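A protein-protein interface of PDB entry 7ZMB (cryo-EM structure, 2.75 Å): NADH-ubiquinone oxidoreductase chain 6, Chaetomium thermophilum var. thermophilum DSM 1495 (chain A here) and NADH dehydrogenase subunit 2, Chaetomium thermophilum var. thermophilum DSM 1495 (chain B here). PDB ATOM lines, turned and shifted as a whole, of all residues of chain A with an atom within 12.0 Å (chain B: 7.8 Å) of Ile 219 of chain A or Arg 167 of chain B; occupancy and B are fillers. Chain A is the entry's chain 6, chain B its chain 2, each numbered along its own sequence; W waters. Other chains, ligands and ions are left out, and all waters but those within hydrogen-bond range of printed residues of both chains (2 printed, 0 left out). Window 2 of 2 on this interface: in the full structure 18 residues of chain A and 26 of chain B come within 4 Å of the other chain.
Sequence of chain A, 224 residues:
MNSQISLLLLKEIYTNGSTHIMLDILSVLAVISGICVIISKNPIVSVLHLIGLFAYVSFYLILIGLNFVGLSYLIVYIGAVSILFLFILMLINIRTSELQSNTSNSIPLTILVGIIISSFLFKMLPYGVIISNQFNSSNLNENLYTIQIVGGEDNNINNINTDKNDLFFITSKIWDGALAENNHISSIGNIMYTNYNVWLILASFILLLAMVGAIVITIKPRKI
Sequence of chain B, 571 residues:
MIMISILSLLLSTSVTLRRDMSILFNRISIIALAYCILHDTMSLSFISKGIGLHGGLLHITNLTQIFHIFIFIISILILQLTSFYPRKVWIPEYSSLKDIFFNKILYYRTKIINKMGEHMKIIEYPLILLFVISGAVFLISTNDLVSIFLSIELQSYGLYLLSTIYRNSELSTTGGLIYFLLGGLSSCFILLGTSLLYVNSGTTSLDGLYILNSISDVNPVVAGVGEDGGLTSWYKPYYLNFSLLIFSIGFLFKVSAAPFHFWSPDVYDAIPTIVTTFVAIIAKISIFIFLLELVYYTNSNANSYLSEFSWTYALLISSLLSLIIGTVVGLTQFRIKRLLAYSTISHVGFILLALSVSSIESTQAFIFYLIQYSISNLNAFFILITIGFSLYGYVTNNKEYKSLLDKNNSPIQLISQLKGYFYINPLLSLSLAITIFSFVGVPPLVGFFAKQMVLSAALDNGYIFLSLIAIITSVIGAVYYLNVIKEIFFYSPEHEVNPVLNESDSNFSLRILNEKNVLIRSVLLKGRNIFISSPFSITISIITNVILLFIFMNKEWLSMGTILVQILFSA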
ATOM      1  N   PHE A  87      28.526  18.853   3.282  1.00  0.00           N
ATOM      2  CA  PHE A  87      28.579  18.763   4.735  1.00  0.00           C
ATOM      3  C   PHE A  87      28.527  20.128   5.400  1.00  0.00           C
ATOM      4  O   PHE A  87      28.020  20.241   6.517  1.00  0.00           O
ATOM      5  CB  PHE A  87      29.825  18.000   5.163  1.00  0.00           C
ATOM      6  CG  PHE A  87      29.656  16.523   5.113  1.00  0.00           C
ATOM      7  CD1 PHE A  87      29.806  15.840   3.924  1.00  0.00           C
ATOM      8  CD2 PHE A  87      29.334  15.810   6.251  1.00  0.00           C
ATOM      9  CE1 PHE A  87      29.645  14.485   3.871  1.00  0.00           C
ATOM     10  CE2 PHE A  87      29.169  14.443   6.193  1.00  0.00           C
ATOM     11  CZ  PHE A  87      29.323  13.786   5.005  1.00  0.00           C
ATOM     12  N   MET A  90      24.863  20.983   5.865  1.00  0.00           N
ATOM     13  CA  MET A  90      24.207  20.224   6.920  1.00  0.00           C
ATOM     14  C   MET A  90      24.701  20.586   8.318  1.00  0.00           C
ATOM     15  O   MET A  90      23.913  20.562   9.265  1.00  0.00           O
ATOM     16  CB  MET A  90      24.407  18.731   6.653  1.00  0.00           C
ATOM     17  CG  MET A  90      23.847  17.805   7.693  1.00  0.00           C
ATOM     18  SD  MET A  90      23.810  16.115   7.093  1.00  0.00           S
ATOM     19  CE  MET A  90      25.552  15.799   6.851  1.00  0.00           C
ATOM     20  N   LEU A  91      25.981  20.928   8.478  1.00  0.00           N
ATOM     21  CA  LEU A  91      26.600  20.992   9.797  1.00  0.00           C
ATOM     22  C   LEU A  91      27.043  22.382  10.227  1.00  0.00           C
ATOM     23  O   LEU A  91      27.572  22.527  11.335  1.00  0.00           O
ATOM     24  CB  LEU A  91      27.818  20.061   9.861  1.00  0.00           C
ATOM     25  CG  LEU A  91      27.638  18.592   9.501  1.00  0.00           C
ATOM     26  CD1 LEU A  91      28.956  17.860   9.644  1.00  0.00           C
ATOM     27  CD2 LEU A  91      26.576  17.961  10.366  1.00  0.00           C
ATOM     28  N   ALA A 210      37.828   2.631   6.136  1.00  0.00           N
ATOM     29  CA  ALA A 210      37.046   3.876   5.966  1.00  0.00           C
ATOM     30  C   ALA A 210      35.606   3.573   5.526  1.00  0.00           C
ATOM     31  O   ALA A 210      34.697   4.214   6.054  1.00  0.00           O
ATOM     32  CB  ALA A 210      37.750   4.796   5.015  1.00  0.00           C
ATOM     33  N   MET A 211      35.407   2.625   4.609  1.00  0.00           N
ATOM     34  CA  MET A 211      34.049   2.227   4.144  1.00  0.00           C
ATOM     35  C   MET A 211      33.252   1.620   5.304  1.00  0.00           C
ATOM     36  O   MET A 211      32.053   1.890   5.388  1.00  0.00           O
ATOM     37  CB  MET A 211      34.126   1.228   2.983  1.00  0.00           C
ATOM     38  CG  MET A 211      34.699   1.798   1.708  1.00  0.00           C
ATOM     39  SD  MET A 211      34.866   0.555   0.405  1.00  0.00           S
ATOM     40  CE  MET A 211      33.151   0.319  -0.052  1.00  0.00           C
ATOM     41  N   VAL A 212      33.896   0.833   6.163  1.00  0.00           N
ATOM     42  CA  VAL A 212      33.220   0.211   7.342  1.00  0.00           C
ATOM     43  C   VAL A 212      33.136   1.215   8.493  1.00  0.00           C
ATOM     44  O   VAL A 212      32.048   1.327   9.073  1.00  0.00           O
ATOM     45  CB  VAL A 212      33.920  -1.094   7.777  1.00  0.00           C
ATOM     46  CG1 VAL A 212      33.388  -1.627   9.098  1.00  0.00           C
ATOM     47  CG2 VAL A 212      33.837  -2.154   6.693  1.00  0.00           C
ATOM     48  N   GLY A 213      34.222   1.927   8.802  1.00  0.00           N
ATOM     49  CA  GLY A 213      34.194   2.810   9.953  1.00  0.00           C
ATOM     50  C   GLY A 213      33.314   4.027   9.748  1.00  0.00           C
ATOM     51  O   GLY A 213      32.534   4.395  10.627  1.00  0.00           O
ATOM     52  N   ALA A 214      33.433   4.676   8.590  1.00  0.00           N
ATOM     53  CA  ALA A 214      32.656   5.887   8.355  1.00  0.00           C
ATOM     54  C   ALA A 214      31.160   5.613   8.357  1.00  0.00           C
ATOM     55  O   ALA A 214      30.371   6.541   8.546  1.00  0.00           O
ATOM     56  CB  ALA A 214      33.071   6.544   7.036  1.00  0.00           C
ATOM     57  N   ILE A 215      30.778   4.353   8.189  1.00  0.00           N
ATOM     58  CA  ILE A 215      29.338   3.979   8.135  1.00  0.00           C
ATOM     59  C   ILE A 215      28.897   3.511   9.521  1.00  0.00           C
ATOM     60  O   ILE A 215      27.763   3.811   9.902  1.00  0.00           O
ATOM     61  CB  ILE A 215      29.109   2.917   7.040  1.00  0.00           C
ATOM     62  CG1 ILE A 215      29.432   3.487   5.658  1.00  0.00           C
ATOM     63  CG2 ILE A 215      27.705   2.337   7.103  1.00  0.00           C
ATOM     64  CD1 ILE A 215      28.909   4.884   5.426  1.00  0.00           C
ATOM     65  N   VAL A 216      29.782   2.833  10.258  1.00  0.00           N
ATOM     66  CA  VAL A 216      29.437   2.321  11.616  1.00  0.00           C
ATOM     67  C   VAL A 216      29.084   3.512  12.514  1.00  0.00           C
ATOM     68  O   VAL A 216      28.142   3.378  13.306  1.00  0.00           O
ATOM     69  CB  VAL A 216      30.533   1.418  12.220  1.00  0.00           C
ATOM     70  CG1 VAL A 216      31.759   2.181  12.684  1.00  0.00           C
ATOM     71  CG2 VAL A 216      29.991   0.578  13.362  1.00  0.00           C
ATOM     72  N   ILE A 217      29.772   4.643  12.351  1.00  0.00           N
ATOM     73  CA  ILE A 217      29.575   5.789  13.285  1.00  0.00           C
ATOM     74  C   ILE A 217      28.445   6.722  12.846  1.00  0.00           C
ATOM     75  O   ILE A 217      28.070   7.574  13.667  1.00  0.00           O
ATOM     76  CB  ILE A 217      30.900   6.537  13.476  1.00  0.00           C
ATOM     77  CG1 ILE A 217      31.437   7.088  12.154  1.00  0.00           C
ATOM     78  CG2 ILE A 217      31.917   5.643  14.169  1.00  0.00           C
ATOM     79  CD1 ILE A 217      32.854   7.588  12.237  1.00  0.00           C
ATOM     80  N   THR A 218      27.931   6.589  11.620  1.00  0.00           N
ATOM     81  CA  THR A 218      26.909   7.560  11.143  1.00  0.00           C
ATOM     82  C   THR A 218      25.641   6.867  10.656  1.00  0.00           C
ATOM     83  O   THR A 218      24.798   7.569  10.096  1.00  0.00           O
ATOM     84  CB  THR A 218      27.436   8.415   9.987  1.00  0.00           C
ATOM     85  OG1 THR A 218      27.750   7.539   8.905  1.00  0.00           O
ATOM     86  CG2 THR A 218      28.643   9.245  10.356  1.00  0.00           C
ATOM     87  N   ILE A 219      25.466   5.589  10.939  1.00  0.00           N
ATOM     88  CA  ILE A 219      24.324   4.847  10.345  1.00  0.00           C
ATOM     89  C   ILE A 219      23.079   5.113  11.172  1.00  0.00           C
ATOM     90  O   ILE A 219      23.176   5.234  12.395  1.00  0.00           O
ATOM     91  CB  ILE A 219      24.628   3.339  10.201  1.00  0.00           C
ATOM     92  CG1 ILE A 219      23.698   2.663   9.191  1.00  0.00           C
ATOM     93  CG2 ILE A 219      24.632   2.621  11.540  1.00  0.00           C
ATOM     94  CD1 ILE A 219      23.721   3.310   7.831  1.00  0.00           C
ATOM     95  N   LYS A 220      21.945   5.221  10.499  1.00  0.00           N
ATOM     96  CA  LYS A 220      20.714   5.388  11.252  1.00  0.00           C
ATOM     97  C   LYS A 220      20.502   4.176  12.152  1.00  0.00           C
ATOM     98  O   LYS A 220      20.612   3.034  11.684  1.00  0.00           O
ATOM     99  CB  LYS A 220      19.520   5.562  10.313  1.00  0.00           C
ATOM    100  CG  LYS A 220      19.755   6.532   9.168  1.00  0.00           C
ATOM    101  CD  LYS A 220      19.840   7.972   9.649  1.00  0.00           C
ATOM    102  CE  LYS A 220      18.460   8.585   9.811  1.00  0.00           C
ATOM    103  NZ  LYS A 220      18.526  10.044  10.098  1.00  0.00           N
ATOM    104  N   PRO A 221      20.214   4.370  13.434  1.00  0.00           N
ATOM    105  CA  PRO A 221      20.054   3.221  14.333  1.00  0.00           C
ATOM    106  C   PRO A 221      18.659   2.619  14.266  1.00  0.00           C
ATOM    107  O   PRO A 221      17.692   3.210  14.756  1.00  0.00           O
ATOM    108  CB  PRO A 221      20.352   3.815  15.713  1.00  0.00           C
ATOM    109  CG  PRO A 221      20.023   5.282  15.585  1.00  0.00           C
ATOM    110  CD  PRO A 221      19.980   5.651  14.119  1.00  0.00           C
ATOM    111  N   ARG A 222      18.546   1.441  13.663  1.00  0.00           N
ATOM    112  CA  ARG A 222      17.264   0.757  13.545  1.00  0.00           C
ATOM    113  C   ARG A 222      17.463  -0.744  13.369  1.00  0.00           C
ATOM    114  O   ARG A 222      17.986  -1.194  12.351  1.00  0.00           O
ATOM    115  CB  ARG A 222      16.458   1.321  12.374  1.00  0.00           C
ATOM    116  N   LEU B  17      22.381  -7.600  11.045  1.00  0.00           N
ATOM    117  CA  LEU B  17      22.251  -6.453  11.934  1.00  0.00           C
ATOM    118  C   LEU B  17      21.839  -6.881  13.337  1.00  0.00           C
ATOM    119  O   LEU B  17      21.333  -6.062  14.110  1.00  0.00           O
ATOM    120  CB  LEU B  17      21.271  -5.418  11.375  1.00  0.00           C
ATOM    121  CG  LEU B  17      21.773  -4.402  10.341  1.00  0.00           C
ATOM    122  CD1 LEU B  17      22.838  -3.494  10.954  1.00  0.00           C
ATOM    123  CD2 LEU B  17      22.285  -5.042   9.071  1.00  0.00           C
ATOM    124  N   GLU B 118      26.446  -1.780  26.453  1.00  0.00           N
ATOM    125  CA  GLU B 118      27.008  -1.174  25.216  1.00  0.00           C
ATOM    126  C   GLU B 118      28.226  -1.949  24.703  1.00  0.00           C
ATOM    127  O   GLU B 118      28.339  -2.104  23.478  1.00  0.00           O
ATOM    128  CB  GLU B 118      27.303   0.308  25.429  1.00  0.00           C
ATOM    129  CG  GLU B 118      27.031   1.136  24.186  1.00  0.00           C
ATOM    130  CD  GLU B 118      25.683   0.857  23.544  1.00  0.00           C
ATOM    131  OE1 GLU B 118      25.665   0.341  22.410  1.00  0.00           O
ATOM    132  OE2 GLU B 118      24.653   1.157  24.181  1.00  0.00           O
ATOM    133  N   ILE B 122      28.103  -3.661  20.168  1.00  0.00           N
ATOM    134  CA  ILE B 122      28.754  -3.137  18.927  1.00  0.00           C
ATOM    135  C   ILE B 122      29.325  -4.299  18.116  1.00  0.00           C
ATOM    136  O   ILE B 122      30.373  -4.818  18.510  1.00  0.00           O
ATOM    137  CB  ILE B 122      29.787  -2.040  19.250  1.00  0.00           C
ATOM    138  CG1 ILE B 122      29.170  -0.945  20.124  1.00  0.00           C
ATOM    139  CG2 ILE B 122      30.387  -1.475  17.976  1.00  0.00           C
ATOM    140  CD1 ILE B 122      30.165   0.053  20.649  1.00  0.00           C
ATOM    141  N   GLU B 124      30.693  -4.437  15.026  1.00  0.00           N
ATOM    142  CA  GLU B 124      31.925  -4.177  14.238  1.00  0.00           C
ATOM    143  C   GLU B 124      33.137  -3.942  15.147  1.00  0.00           C
ATOM    144  O   GLU B 124      34.234  -3.798  14.609  1.00  0.00           O
ATOM    145  CB  GLU B 124      31.700  -3.001  13.279  1.00  0.00           C
ATOM    146  CG  GLU B 124      30.519  -3.171  12.338  1.00  0.00           C
ATOM    147  CD  GLU B 124      29.141  -2.801  12.870  1.00  0.00           C
ATOM    148  OE1 GLU B 124      28.197  -2.768  12.064  1.00  0.00           O
ATOM    149  OE2 GLU B 124      29.011  -2.545  14.083  1.00  0.00           O
ATOM    150  N   LEU B 161      38.454   5.511  14.874  1.00  0.00           N
ATOM    151  CA  LEU B 161      37.121   4.927  14.784  1.00  0.00           C
ATOM    152  C   LEU B 161      36.757   4.183  16.058  1.00  0.00           C
ATOM    153  O   LEU B 161      35.590   4.176  16.466  1.00  0.00           O
ATOM    154  CB  LEU B 161      37.027   3.995  13.581  1.00  0.00           C
ATOM    155  CG  LEU B 161      37.204   4.633  12.206  1.00  0.00           C
ATOM    156  CD1 LEU B 161      37.435   3.553  11.189  1.00  0.00           C
ATOM    157  CD2 LEU B 161      36.012   5.494  11.829  1.00  0.00           C
ATOM    158  N   LEU B 162      37.736   3.538  16.692  1.00  0.00           N
ATOM    159  CA  LEU B 162      37.493   2.927  17.990  1.00  0.00           C
ATOM    160  C   LEU B 162      37.168   3.978  19.043  1.00  0.00           C
ATOM    161  O   LEU B 162      36.273   3.778  19.868  1.00  0.00           O
ATOM    162  CB  LEU B 162      38.702   2.100  18.412  1.00  0.00           C
ATOM    163  CG  LEU B 162      38.800   0.652  17.947  1.00  0.00           C
ATOM    164  CD1 LEU B 162      39.859  -0.048  18.760  1.00  0.00           C
ATOM    165  CD2 LEU B 162      37.474  -0.061  18.074  1.00  0.00           C
ATOM    166  N   SER B 163      37.888   5.102  19.035  1.00  0.00           N
ATOM    167  CA  SER B 163      37.598   6.192  19.959  1.00  0.00           C
ATOM    168  C   SER B 163      36.225   6.799  19.723  1.00  0.00           C
ATOM    169  O   SER B 163      35.716   7.511  20.589  1.00  0.00           O
ATOM    170  CB  SER B 163      38.658   7.289  19.841  1.00  0.00           C
ATOM    171  OG  SER B 163      39.954   6.797  20.110  1.00  0.00           O
ATOM    172  N   THR B 164      35.608   6.529  18.569  1.00  0.00           N
ATOM    173  CA  THR B 164      34.306   7.157  18.216  1.00  0.00           C
ATOM    174  C   THR B 164      33.212   6.096  18.070  1.00  0.00           C
ATOM    175  O   THR B 164      32.082   6.484  17.773  1.00  0.00           O
ATOM    176  CB  THR B 164      34.427   7.902  16.878  1.00  0.00           C
ATOM    177  OG1 THR B 164      35.543   8.788  16.955  1.00  0.00           O
ATOM    178  CG2 THR B 164      33.176   8.670  16.508  1.00  0.00           C
ATOM    179  N   ILE B 165      33.523   4.814  18.272  1.00  0.00           N
ATOM    180  CA  ILE B 165      32.541   3.725  17.979  1.00  0.00           C
ATOM    181  C   ILE B 165      31.370   3.781  18.959  1.00  0.00           C
ATOM    182  O   ILE B 165      30.309   3.224  18.632  1.00  0.00           O
ATOM    183  CB  ILE B 165      33.250   2.355  17.942  1.00  0.00           C
ATOM    184  CG1 ILE B 165      32.586   1.388  16.959  1.00  0.00           C
ATOM    185  CG2 ILE B 165      33.409   1.755  19.330  1.00  0.00           C
ATOM    186  CD1 ILE B 165      33.377   0.131  16.720  1.00  0.00           C
ATOM    187  N   TYR B 166      31.534   4.416  20.124  1.00  0.00           N
ATOM    188  CA  TYR B 166      30.375   4.664  21.034  1.00  0.00           C
ATOM    189  C   TYR B 166      29.804   5.971  20.489  1.00  0.00           C
ATOM    190  O   TYR B 166      30.272   7.033  20.920  1.00  0.00           O
ATOM    191  CB  TYR B 166      30.821   4.713  22.495  1.00  0.00           C
ATOM    192  CG  TYR B 166      31.073   3.372  23.133  1.00  0.00           C
ATOM    193  CD1 TYR B 166      32.109   2.558  22.710  1.00  0.00           C
ATOM    194  CD2 TYR B 166      30.286   2.924  24.178  1.00  0.00           C
ATOM    195  CE1 TYR B 166      32.352   1.330  23.300  1.00  0.00           C
ATOM    196  CE2 TYR B 166      30.517   1.701  24.784  1.00  0.00           C
ATOM    197  CZ  TYR B 166      31.551   0.900  24.341  1.00  0.00           C
ATOM    198  OH  TYR B 166      31.779  -0.305  24.936  1.00  0.00           O
ATOM    199  N   ARG B 167      28.813   5.901  19.607  1.00  0.00           N
ATOM    200  CA  ARG B 167      28.348   7.087  18.844  1.00  0.00           C
ATOM    201  C   ARG B 167      27.268   7.847  19.597  1.00  0.00           C
ATOM    202  O   ARG B 167      26.900   8.935  19.157  1.00  0.00           O
ATOM    203  CB  ARG B 167      27.774   6.538  17.538  1.00  0.00           C
ATOM    204  CG  ARG B 167      26.857   5.348  17.767  1.00  0.00           C
ATOM    205  CD  ARG B 167      26.261   4.889  16.463  1.00  0.00           C
ATOM    206  NE  ARG B 167      25.552   5.989  15.839  1.00  0.00           N
ATOM    207  CZ  ARG B 167      25.185   5.979  14.572  1.00  0.00           C
ATOM    208  NH1 ARG B 167      24.536   7.009  14.055  1.00  0.00           N
ATOM    209  NH2 ARG B 167      25.485   4.934  13.827  1.00  0.00           N
ATOM    210  N   ASN B 168      26.776   7.258  20.680  1.00  0.00           N
ATOM    211  CA  ASN B 168      25.685   7.904  21.452  1.00  0.00           C
ATOM    212  C   ASN B 168      26.293   8.536  22.698  1.00  0.00           C
ATOM    213  O   ASN B 168      25.521   9.046  23.519  1.00  0.00           O
ATOM    214  CB  ASN B 168      24.558   6.900  21.670  1.00  0.00           C
ATOM    215  CG  ASN B 168      24.094   6.251  20.387  1.00  0.00           C
ATOM    216  OD1 ASN B 168      24.046   6.893  19.342  1.00  0.00           O
ATOM    217  ND2 ASN B 168      23.739   4.980  20.461  1.00  0.00           N
ATOM    218  N   SER B 169      27.619   8.512  22.781  1.00  0.00           N
ATOM    219  CA  SER B 169      28.342   9.173  23.890  1.00  0.00           C
ATOM    220  C   SER B 169      28.906  10.496  23.382  1.00  0.00           C
ATOM    221  O   SER B 169      29.706  10.459  22.443  1.00  0.00           O
ATOM    222  CB  SER B 169      29.430   8.282  24.394  1.00  0.00           C
ATOM    223  OG  SER B 169      30.247   8.956  25.332  1.00  0.00           O
ATOM    224  N   GLU B 170      28.497  11.620  23.973  1.00  0.00           N
ATOM    225  CA  GLU B 170      29.062  12.952  23.613  1.00  0.00           C
ATOM    226  C   GLU B 170      30.517  13.007  24.065  1.00  0.00           C
ATOM    227  O   GLU B 170      31.274  13.808  23.513  1.00  0.00           O
ATOM    228  CB  GLU B 170      28.255  14.110  24.202  1.00  0.00           C
ATOM    229  CG  GLU B 170      28.069  14.033  25.706  1.00  0.00           C
ATOM    230  CD  GLU B 170      26.922  13.145  26.162  1.00  0.00           C
ATOM    231  OE1 GLU B 170      27.186  11.987  26.545  1.00  0.00           O
ATOM    232  OE2 GLU B 170      25.768  13.612  26.122  1.00  0.00           O
ATOM    233  N   LEU B 171      30.899  12.121  24.982  1.00  0.00           N
ATOM    234  CA  LEU B 171      32.271  12.145  25.533  1.00  0.00           C
ATOM    235  C   LEU B 171      33.197  11.377  24.592  1.00  0.00           C
ATOM    236  O   LEU B 171      34.354  11.773  24.478  1.00  0.00           O
ATOM    237  CB  LEU B 171      32.289  11.581  26.955  1.00  0.00           C
ATOM    238  CG  LEU B 171      32.049  12.582  28.073  1.00  0.00           C
ATOM    239  CD1 LEU B 171      32.339  11.944  29.421  1.00  0.00           C
ATOM    240  CD2 LEU B 171      32.919  13.803  27.868  1.00  0.00           C
ATOM    241  N   SER B 172      32.685  10.345  23.917  1.00  0.00           N
ATOM    242  CA  SER B 172      33.526   9.590  22.998  1.00  0.00           C
ATOM    243  C   SER B 172      33.680  10.301  21.665  1.00  0.00           C
ATOM    244  O   SER B 172      34.762  10.280  21.072  1.00  0.00           O
ATOM    245  CB  SER B 172      32.962   8.192  22.778  1.00  0.00           C
ATOM    246  OG  SER B 172      33.121   7.418  23.940  1.00  0.00           O
ATOM    247  N   THR B 173      32.615  10.946  21.237  1.00  0.00           N
ATOM    248  CA  THR B 173      32.617  11.696  19.961  1.00  0.00           C
ATOM    249  C   THR B 173      33.637  12.816  20.096  1.00  0.00           C
ATOM    250  O   THR B 173      34.304  13.109  19.112  1.00  0.00           O
ATOM    251  CB  THR B 173      31.196  12.061  19.531  1.00  0.00           C
ATOM    252  OG1 THR B 173      30.538  12.727  20.606  1.00  0.00           O
ATOM    253  CG2 THR B 173      30.405  10.848  19.095  1.00  0.00           C
ATOM    254  N   ASN B 409      29.988   4.049  30.616  1.00  0.00           N
ATOM    255  CA  ASN B 409      31.183   3.834  29.816  1.00  0.00           C
ATOM    256  C   ASN B 409      32.461   3.919  30.630  1.00  0.00           C
ATOM    257  O   ASN B 409      33.449   3.264  30.290  1.00  0.00           O
ATOM    258  CB  ASN B 409      31.238   4.846  28.671  1.00  0.00           C
ATOM    259  CG  ASN B 409      30.200   4.584  27.616  1.00  0.00           C
ATOM    260  OD1 ASN B 409      29.727   3.464  27.461  1.00  0.00           O
ATOM    261  ND2 ASN B 409      29.835   5.620  26.876  1.00  0.00           N
HETATM  262  O   HOH W   1      26.493   9.073  15.188  1.00  0.00           O
HETATM  263  O   HOH W   2      29.065   2.976  16.098  1.00  0.00           O
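The guanidinium group (NH2) of Arg 167 of chain B sits at hydrogen-bond distance from the backbone carbonyl oxygen (O) of Val 216 of chain A (3.1 Å).
NH2 of Arg 167 of chain B is in hydrogen-bond range of O of Ile 219 of chain A, 2.7 Å away.
The side-chain hydroxyl (OG1) of Thr 218 of chain A sits at hydrogen-bond distance from the backbone carbonyl oxygen (O) of Ala 214 of chain A (2.8 Å).
Among the printed residues, merely in contact across the chains: Val 216 of chain A with Glu 124 of chain B (3.4 Å), Ile 217 of chain A with Arg 167 of chain B (3.4 Å), Gly 213 of chain A with Leu 161 of chain B (3.5 Å), Thr 218 of chain A with Arg 167 of chain B (3.6 Å), Ile 217 of chain A with Thr 164 of chain B (3.7 Å) and Ile 217 of chain A with Leu 161 of chain B (3.8 Å).
Of the printed residues of chain B, Val 216 of chain A touches Glu 124 (3.4 Å) and Arg 167 (3.1 Å).
Of the printed residues of chain B, Thr 218 of chain A touches Arg 167.
Ile 219 of chain A touches just one residue of chain B: Arg 167 (2.7 Å).
Of the printed residues of chain A, Leu 161 of chain B touches Gly 213 and Ile 217.
Of chain A, only Ile 217 (3.7 Å) comes within 4 Å of Thr 164 of chain B.
No residue of chain A comes within 4 Å of Ile 165 of chain B.
No residue of chain A comes within 4 Å of Ser 169 of chain B.
No residue of chain A comes within 4 Å of Ser 172 of chain B.
Hydrophobic or aromatic side chains of chain B that line the printed part of chain A: Leu 161.
Hydrophobic or aromatic side chains of chain A that line the printed part of chain B: Val 216, Ile 217 and Ile 219.
Among the printed residues, 8 pairs touch across the chains.
Among the printed residues, no Asp or Glu carboxylate lies within 4 Å of a Lys or Arg side-chain nitrogen of the other chain.
Water W1 lies within hydrogen-bond range of O of Ile 217 of chain A (2.7 Å) and NH1 of Arg 167 of chain B (3.1 Å).
Water W2 bridges O of Ile 165 of chain B (2.8 Å) and O of Val 216 of chain A (3.0 Å).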
